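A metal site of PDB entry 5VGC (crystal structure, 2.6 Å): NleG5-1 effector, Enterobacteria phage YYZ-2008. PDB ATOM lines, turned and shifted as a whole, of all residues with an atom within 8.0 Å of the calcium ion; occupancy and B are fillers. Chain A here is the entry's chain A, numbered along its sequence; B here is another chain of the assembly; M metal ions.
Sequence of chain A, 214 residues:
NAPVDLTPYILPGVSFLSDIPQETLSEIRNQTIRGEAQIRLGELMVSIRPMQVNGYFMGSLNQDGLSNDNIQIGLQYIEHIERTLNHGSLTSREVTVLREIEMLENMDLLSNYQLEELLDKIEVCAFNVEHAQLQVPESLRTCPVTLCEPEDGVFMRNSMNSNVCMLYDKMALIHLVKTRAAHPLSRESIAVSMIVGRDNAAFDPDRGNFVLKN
OE2 of Glu 102 of chain A is in salt-bridge range of NH1 of Arg 99 of chain A, at 3.6 Å. OE1 of Glu 102 of chain A is in hydrogen-bond range of N of Asp 108 of chain B (3.2 Å). OE2 of Glu 102 of chain B lies within salt-bridge range of NH1 of Arg 99 of chain B (3.6 Å). The side-chain carboxylate of Glu 102 of chain B lies within hydrogen-bond range of the backbone NH of Asp 108 of chain A (3.2 Å).
Within 4 Å of the calcium ion: Glu 102 of chain A, Leu 104 of chain A, Glu 102 of chain B and Leu 104 of chain B.
The calcium ion is bound by the backbone carbonyl oxygen (O) of Leu 104 of chain A, 2.3 Å away. The calcium ion is bound by the backbone carbonyl oxygen (O) of Leu 104 of chain B (2.3 Å). O of Glu 102 of chain A binds the calcium ion, 2.3 Å away. The calcium ion is bound by O of Glu 102 of chain B, at 2.6 Å.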
ATOM      1  N   ARG A  99      -0.832 -25.918  16.054  1.00  0.00           N
ATOM      2  CA  ARG A  99      -0.916 -25.430  14.676  1.00  0.00           C
ATOM      3  C   ARG A  99       0.298 -24.553  14.320  1.00  0.00           C
ATOM      4  O   ARG A  99       0.823 -24.662  13.200  1.00  0.00           O
ATOM      5  CB  ARG A  99      -2.221 -24.660  14.460  1.00  0.00           C
ATOM      6  CG  ARG A  99      -2.585 -24.441  13.001  1.00  0.00           C
ATOM      7  CD  ARG A  99      -3.156 -25.701  12.387  1.00  0.00           C
ATOM      8  NE  ARG A  99      -3.488 -25.473  10.991  1.00  0.00           N
ATOM      9  CZ  ARG A  99      -2.610 -25.489   9.986  1.00  0.00           C
ATOM     10  NH1 ARG A  99      -1.321 -25.726  10.175  1.00  0.00           N
ATOM     11  NH2 ARG A  99      -3.047 -25.269   8.741  1.00  0.00           N
ATOM     12  N   GLU A 100       0.730 -23.701  15.258  1.00  0.00           N
ATOM     13  CA  GLU A 100       1.952 -22.914  15.056  1.00  0.00           C
ATOM     14  C   GLU A 100       3.144 -23.829  14.860  1.00  0.00           C
ATOM     15  O   GLU A 100       3.980 -23.570  13.979  1.00  0.00           O
ATOM     16  CB  GLU A 100       2.215 -21.953  16.215  1.00  0.00           C
ATOM     17  CG  GLU A 100       1.246 -20.780  16.312  1.00  0.00           C
ATOM     18  CD  GLU A 100       1.452 -19.710  15.265  1.00  0.00           C
ATOM     19  OE1 GLU A 100       2.385 -19.834  14.424  1.00  0.00           O
ATOM     20  OE2 GLU A 100       0.666 -18.747  15.291  1.00  0.00           O
ATOM     21  N   ILE A 101       3.236 -24.901  15.649  1.00  0.00           N
ATOM     22  CA  ILE A 101       4.307 -25.886  15.366  1.00  0.00           C
ATOM     23  C   ILE A 101       4.166 -26.431  13.951  1.00  0.00           C
ATOM     24  O   ILE A 101       5.138 -26.454  13.206  1.00  0.00           O
ATOM     25  CB  ILE A 101       4.332 -27.061  16.374  1.00  0.00           C
ATOM     26  CG1 ILE A 101       4.728 -26.546  17.750  1.00  0.00           C
ATOM     27  CG2 ILE A 101       5.310 -28.152  15.914  1.00  0.00           C
ATOM     28  CD1 ILE A 101       4.394 -27.495  18.877  1.00  0.00           C
ATOM     29  N   GLU A 102       2.965 -26.876  13.580  1.00  0.00           N
ATOM     30  CA  GLU A 102       2.742 -27.441  12.229  1.00  0.00           C
ATOM     31  C   GLU A 102       3.153 -26.487  11.126  1.00  0.00           C
ATOM     32  O   GLU A 102       3.816 -26.884  10.155  1.00  0.00           O
ATOM     33  CB  GLU A 102       1.266 -27.865  12.043  1.00  0.00           C
ATOM     34  CG  GLU A 102       0.858 -29.117  12.852  1.00  0.00           C
ATOM     35  CD  GLU A 102      -0.618 -29.469  12.746  1.00  0.00           C
ATOM     36  OE1 GLU A 102      -1.004 -30.511  13.328  1.00  0.00           O
ATOM     37  OE2 GLU A 102      -1.394 -28.716  12.102  1.00  0.00           O
ATOM     38  N   MET A 103       2.785 -25.216  11.278  1.00  0.00           N
ATOM     39  CA  MET A 103       3.024 -24.188  10.263  1.00  0.00           C
ATOM     40  C   MET A 103       4.486 -23.770  10.056  1.00  0.00           C
ATOM     41  O   MET A 103       4.772 -22.994   9.161  1.00  0.00           O
ATOM     42  CB  MET A 103       2.175 -22.952  10.546  1.00  0.00           C
ATOM     43  CG  MET A 103       0.714 -23.152  10.203  1.00  0.00           C
ATOM     44  SD  MET A 103      -0.177 -21.595  10.286  1.00  0.00           S
ATOM     45  CE  MET A 103      -0.751 -21.546  11.988  1.00  0.00           C
ATOM     46  N   LEU A 104       5.406 -24.269  10.869  1.00  0.00           N
ATOM     47  CA  LEU A 104       6.837 -24.099  10.584  1.00  0.00           C
ATOM     48  C   LEU A 104       7.144 -24.719   9.226  1.00  0.00           C
ATOM     49  O   LEU A 104       6.577 -25.760   8.884  1.00  0.00           O
ATOM     50  CB  LEU A 104       7.726 -24.733  11.668  1.00  0.00           C
ATOM     51  CG  LEU A 104       7.756 -24.061  13.037  1.00  0.00           C
ATOM     52  CD1 LEU A 104       8.264 -25.014  14.117  1.00  0.00           C
ATOM     53  CD2 LEU A 104       8.609 -22.806  13.010  1.00  0.00           C
ATOM     54  N   GLU A 105       8.044 -24.093   8.483  1.00  0.00           N
ATOM     55  CA  GLU A 105       8.401 -24.475   7.126  1.00  0.00           C
ATOM     56  C   GLU A 105       9.837 -24.958   7.035  1.00  0.00           C
ATOM     57  O   GLU A 105      10.661 -24.746   7.966  1.00  0.00           O
ATOM     58  CB  GLU A 105       8.199 -23.270   6.193  1.00  0.00           C
ATOM     59  CG  GLU A 105       6.795 -22.653   6.295  1.00  0.00           C
ATOM     60  CD  GLU A 105       6.533 -21.539   5.289  1.00  0.00           C
ATOM     61  OE1 GLU A 105       7.452 -20.740   4.974  1.00  0.00           O
ATOM     62  OE2 GLU A 105       5.379 -21.452   4.803  1.00  0.00           O
ATOM     63  N   ASN A 106      10.153 -25.617   5.917  1.00  0.00           N
ATOM     64  CA  ASN A 106      11.497 -26.122   5.670  1.00  0.00           C
ATOM     65  C   ASN A 106      12.530 -25.022   5.956  1.00  0.00           C
ATOM     66  O   ASN A 106      12.360 -23.876   5.556  1.00  0.00           O
ATOM     67  CB  ASN A 106      11.634 -26.663   4.238  1.00  0.00           C
ATOM     68  CG  ASN A 106      10.680 -27.828   3.950  1.00  0.00           C
ATOM     69  OD1 ASN A 106      10.422 -28.681   4.830  1.00  0.00           O
ATOM     70  ND2 ASN A 106      10.156 -27.870   2.730  1.00  0.00           N
ATOM     71  N   ASP A 108      13.006 -23.365   8.668  1.00  0.00           N
ATOM     72  CA  ASP A 108      12.632 -22.299   9.635  1.00  0.00           C
ATOM     73  C   ASP A 108      13.363 -22.442  10.980  1.00  0.00           C
ATOM     74  O   ASP A 108      13.721 -21.428  11.595  1.00  0.00           O
ATOM     75  CB  ASP A 108      11.118 -22.263   9.908  1.00  0.00           C
ATOM     76  CG  ASP A 108      10.362 -21.228   9.062  1.00  0.00           C
ATOM     77  OD1 ASP A 108      10.970 -20.294   8.504  1.00  0.00           O
ATOM     78  OD2 ASP A 108       9.099 -21.338   8.977  1.00  0.00           O
ATOM     79  N   ARG B  99      14.619 -31.148  11.801  1.00  0.00           N
ATOM     80  CA  ARG B  99      14.008 -31.350  10.494  1.00  0.00           C
ATOM     81  C   ARG B  99      12.673 -32.105  10.608  1.00  0.00           C
ATOM     82  O   ARG B  99      11.723 -31.762   9.931  1.00  0.00           O
ATOM     83  CB  ARG B  99      14.967 -32.060   9.545  1.00  0.00           C
ATOM     84  CG  ARG B  99      14.596 -31.942   8.087  1.00  0.00           C
ATOM     85  CD  ARG B  99      14.890 -30.572   7.503  1.00  0.00           C
ATOM     86  NE  ARG B  99      14.511 -30.564   6.091  1.00  0.00           N
ATOM     87  CZ  ARG B  99      13.281 -30.385   5.633  1.00  0.00           C
ATOM     88  NH1 ARG B  99      12.241 -30.185   6.453  1.00  0.00           N
ATOM     89  NH2 ARG B  99      13.073 -30.409   4.318  1.00  0.00           N
ATOM     90  N   GLU B 100      12.628 -33.130  11.459  1.00  0.00           N
ATOM     91  CA  GLU B 100      11.374 -33.851  11.743  1.00  0.00           C
ATOM     92  C   GLU B 100      10.348 -32.896  12.296  1.00  0.00           C
ATOM     93  O   GLU B 100       9.182 -32.962  11.898  1.00  0.00           O
ATOM     94  CB  GLU B 100      11.571 -35.020  12.709  1.00  0.00           C
ATOM     95  CG  GLU B 100      12.318 -36.208  12.131  1.00  0.00           C
ATOM     96  CD  GLU B 100      11.494 -37.045  11.179  1.00  0.00           C
ATOM     97  OE1 GLU B 100      10.295 -36.755  10.964  1.00  0.00           O
ATOM     98  OE2 GLU B 100      12.050 -38.041  10.644  1.00  0.00           O
ATOM     99  N   ILE B 101      10.755 -31.998  13.204  1.00  0.00           N
ATOM    100  CA  ILE B 101       9.787 -30.972  13.641  1.00  0.00           C
ATOM    101  C   ILE B 101       9.292 -30.153  12.436  1.00  0.00           C
ATOM    102  O   ILE B 101       8.070 -30.001  12.247  1.00  0.00           O
ATOM    103  CB  ILE B 101      10.345 -30.015  14.714  1.00  0.00           C
ATOM    104  CG1 ILE B 101      10.615 -30.768  16.002  1.00  0.00           C
ATOM    105  CG2 ILE B 101       9.348 -28.882  14.985  1.00  0.00           C
ATOM    106  CD1 ILE B 101      11.551 -30.045  16.943  1.00  0.00           C
ATOM    107  N   GLU B 102      10.241 -29.644  11.640  1.00  0.00           N
ATOM    108  CA  GLU B 102       9.859 -28.837  10.453  1.00  0.00           C
ATOM    109  C   GLU B 102       8.873 -29.578   9.511  1.00  0.00           C
ATOM    110  O   GLU B 102       7.880 -29.003   9.056  1.00  0.00           O
ATOM    111  CB  GLU B 102      11.106 -28.400   9.664  1.00  0.00           C
ATOM    112  CG  GLU B 102      11.986 -27.360  10.358  1.00  0.00           C
ATOM    113  CD  GLU B 102      13.227 -26.971   9.578  1.00  0.00           C
ATOM    114  OE1 GLU B 102      13.975 -26.082  10.071  1.00  0.00           O
ATOM    115  OE2 GLU B 102      13.448 -27.522   8.467  1.00  0.00           O
ATOM    116  N   MET B 103       9.164 -30.851   9.258  1.00  0.00           N
ATOM    117  CA  MET B 103       8.427 -31.654   8.295  1.00  0.00           C
ATOM    118  C   MET B 103       7.000 -32.032   8.719  1.00  0.00           C
ATOM    119  O   MET B 103       6.279 -32.639   7.906  1.00  0.00           O
ATOM    120  CB  MET B 103       9.176 -32.949   7.981  1.00  0.00           C
ATOM    121  CG  MET B 103      10.368 -32.805   7.073  1.00  0.00           C
ATOM    122  SD  MET B 103      11.051 -34.436   6.723  1.00  0.00           S
ATOM    123  CE  MET B 103      12.614 -34.028   5.959  1.00  0.00           C
ATOM    124  N   LEU B 104       6.587 -31.700   9.950  1.00  0.00           N
ATOM    125  CA  LEU B 104       5.183 -31.841  10.323  1.00  0.00           C
ATOM    126  C   LEU B 104       4.335 -31.006   9.365  1.00  0.00           C
ATOM    127  O   LEU B 104       4.743 -29.908   8.939  1.00  0.00           O
ATOM    128  CB  LEU B 104       4.930 -31.400  11.764  1.00  0.00           C
ATOM    129  CG  LEU B 104       5.470 -32.303  12.886  1.00  0.00           C
ATOM    130  CD1 LEU B 104       5.560 -31.565  14.215  1.00  0.00           C
ATOM    131  CD2 LEU B 104       4.632 -33.573  13.029  1.00  0.00           C
ATOM    132  N   GLU B 105       3.164 -31.564   9.032  1.00  0.00           N
ATOM    133  CA  GLU B 105       2.217 -30.941   8.115  1.00  0.00           C
ATOM    134  C   GLU B 105       0.929 -30.592   8.839  1.00  0.00           C
ATOM    135  O   GLU B 105       0.626 -31.116   9.937  1.00  0.00           O
ATOM    136  CB  GLU B 105       1.917 -31.874   6.926  1.00  0.00           C
ATOM    137  CG  GLU B 105       3.185 -32.385   6.225  1.00  0.00           C
ATOM    138  CD  GLU B 105       2.918 -33.297   5.042  1.00  0.00           C
ATOM    139  OE1 GLU B 105       1.962 -33.033   4.275  1.00  0.00           O
ATOM    140  OE2 GLU B 105       3.680 -34.283   4.884  1.00  0.00           O
ATOM    141  N   ASN B 106       0.164 -29.692   8.206  1.00  0.00           N
ATOM    142  CA  ASN B 106      -1.170 -29.338   8.687  1.00  0.00           C
ATOM    143  C   ASN B 106      -1.953 -30.601   9.117  1.00  0.00           C
ATOM    144  O   ASN B 106      -1.983 -31.609   8.392  1.00  0.00           O
ATOM    145  CB  ASN B 106      -1.963 -28.482   7.677  1.00  0.00           C
ATOM    146  CG  ASN B 106      -1.624 -28.772   6.217  1.00  0.00           C
ATOM    147  OD1 ASN B 106      -0.711 -28.158   5.654  1.00  0.00           O
ATOM    148  ND2 ASN B 106      -2.362 -29.683   5.604  1.00  0.00           N
ATOM    149  N   ASP B 108      -1.147 -32.880  11.234  1.00  0.00           N
ATOM    150  CA  ASP B 108      -0.385 -34.083  11.627  1.00  0.00           C
ATOM    151  C   ASP B 108      -0.451 -34.394  13.129  1.00  0.00           C
ATOM    152  O   ASP B 108      -0.475 -35.556  13.524  1.00  0.00           O
ATOM    153  CB  ASP B 108       1.099 -34.011  11.188  1.00  0.00           C
ATOM    154  CG  ASP B 108       1.390 -34.727   9.860  1.00  0.00           C
ATOM    155  OD1 ASP B 108       0.575 -35.557   9.396  1.00  0.00           O
ATOM    156  OD2 ASP B 108       2.468 -34.455   9.283  1.00  0.00           O
HETATM  157 CA    CA M   1       5.612 -27.802   9.034  1.00  0.00          CA
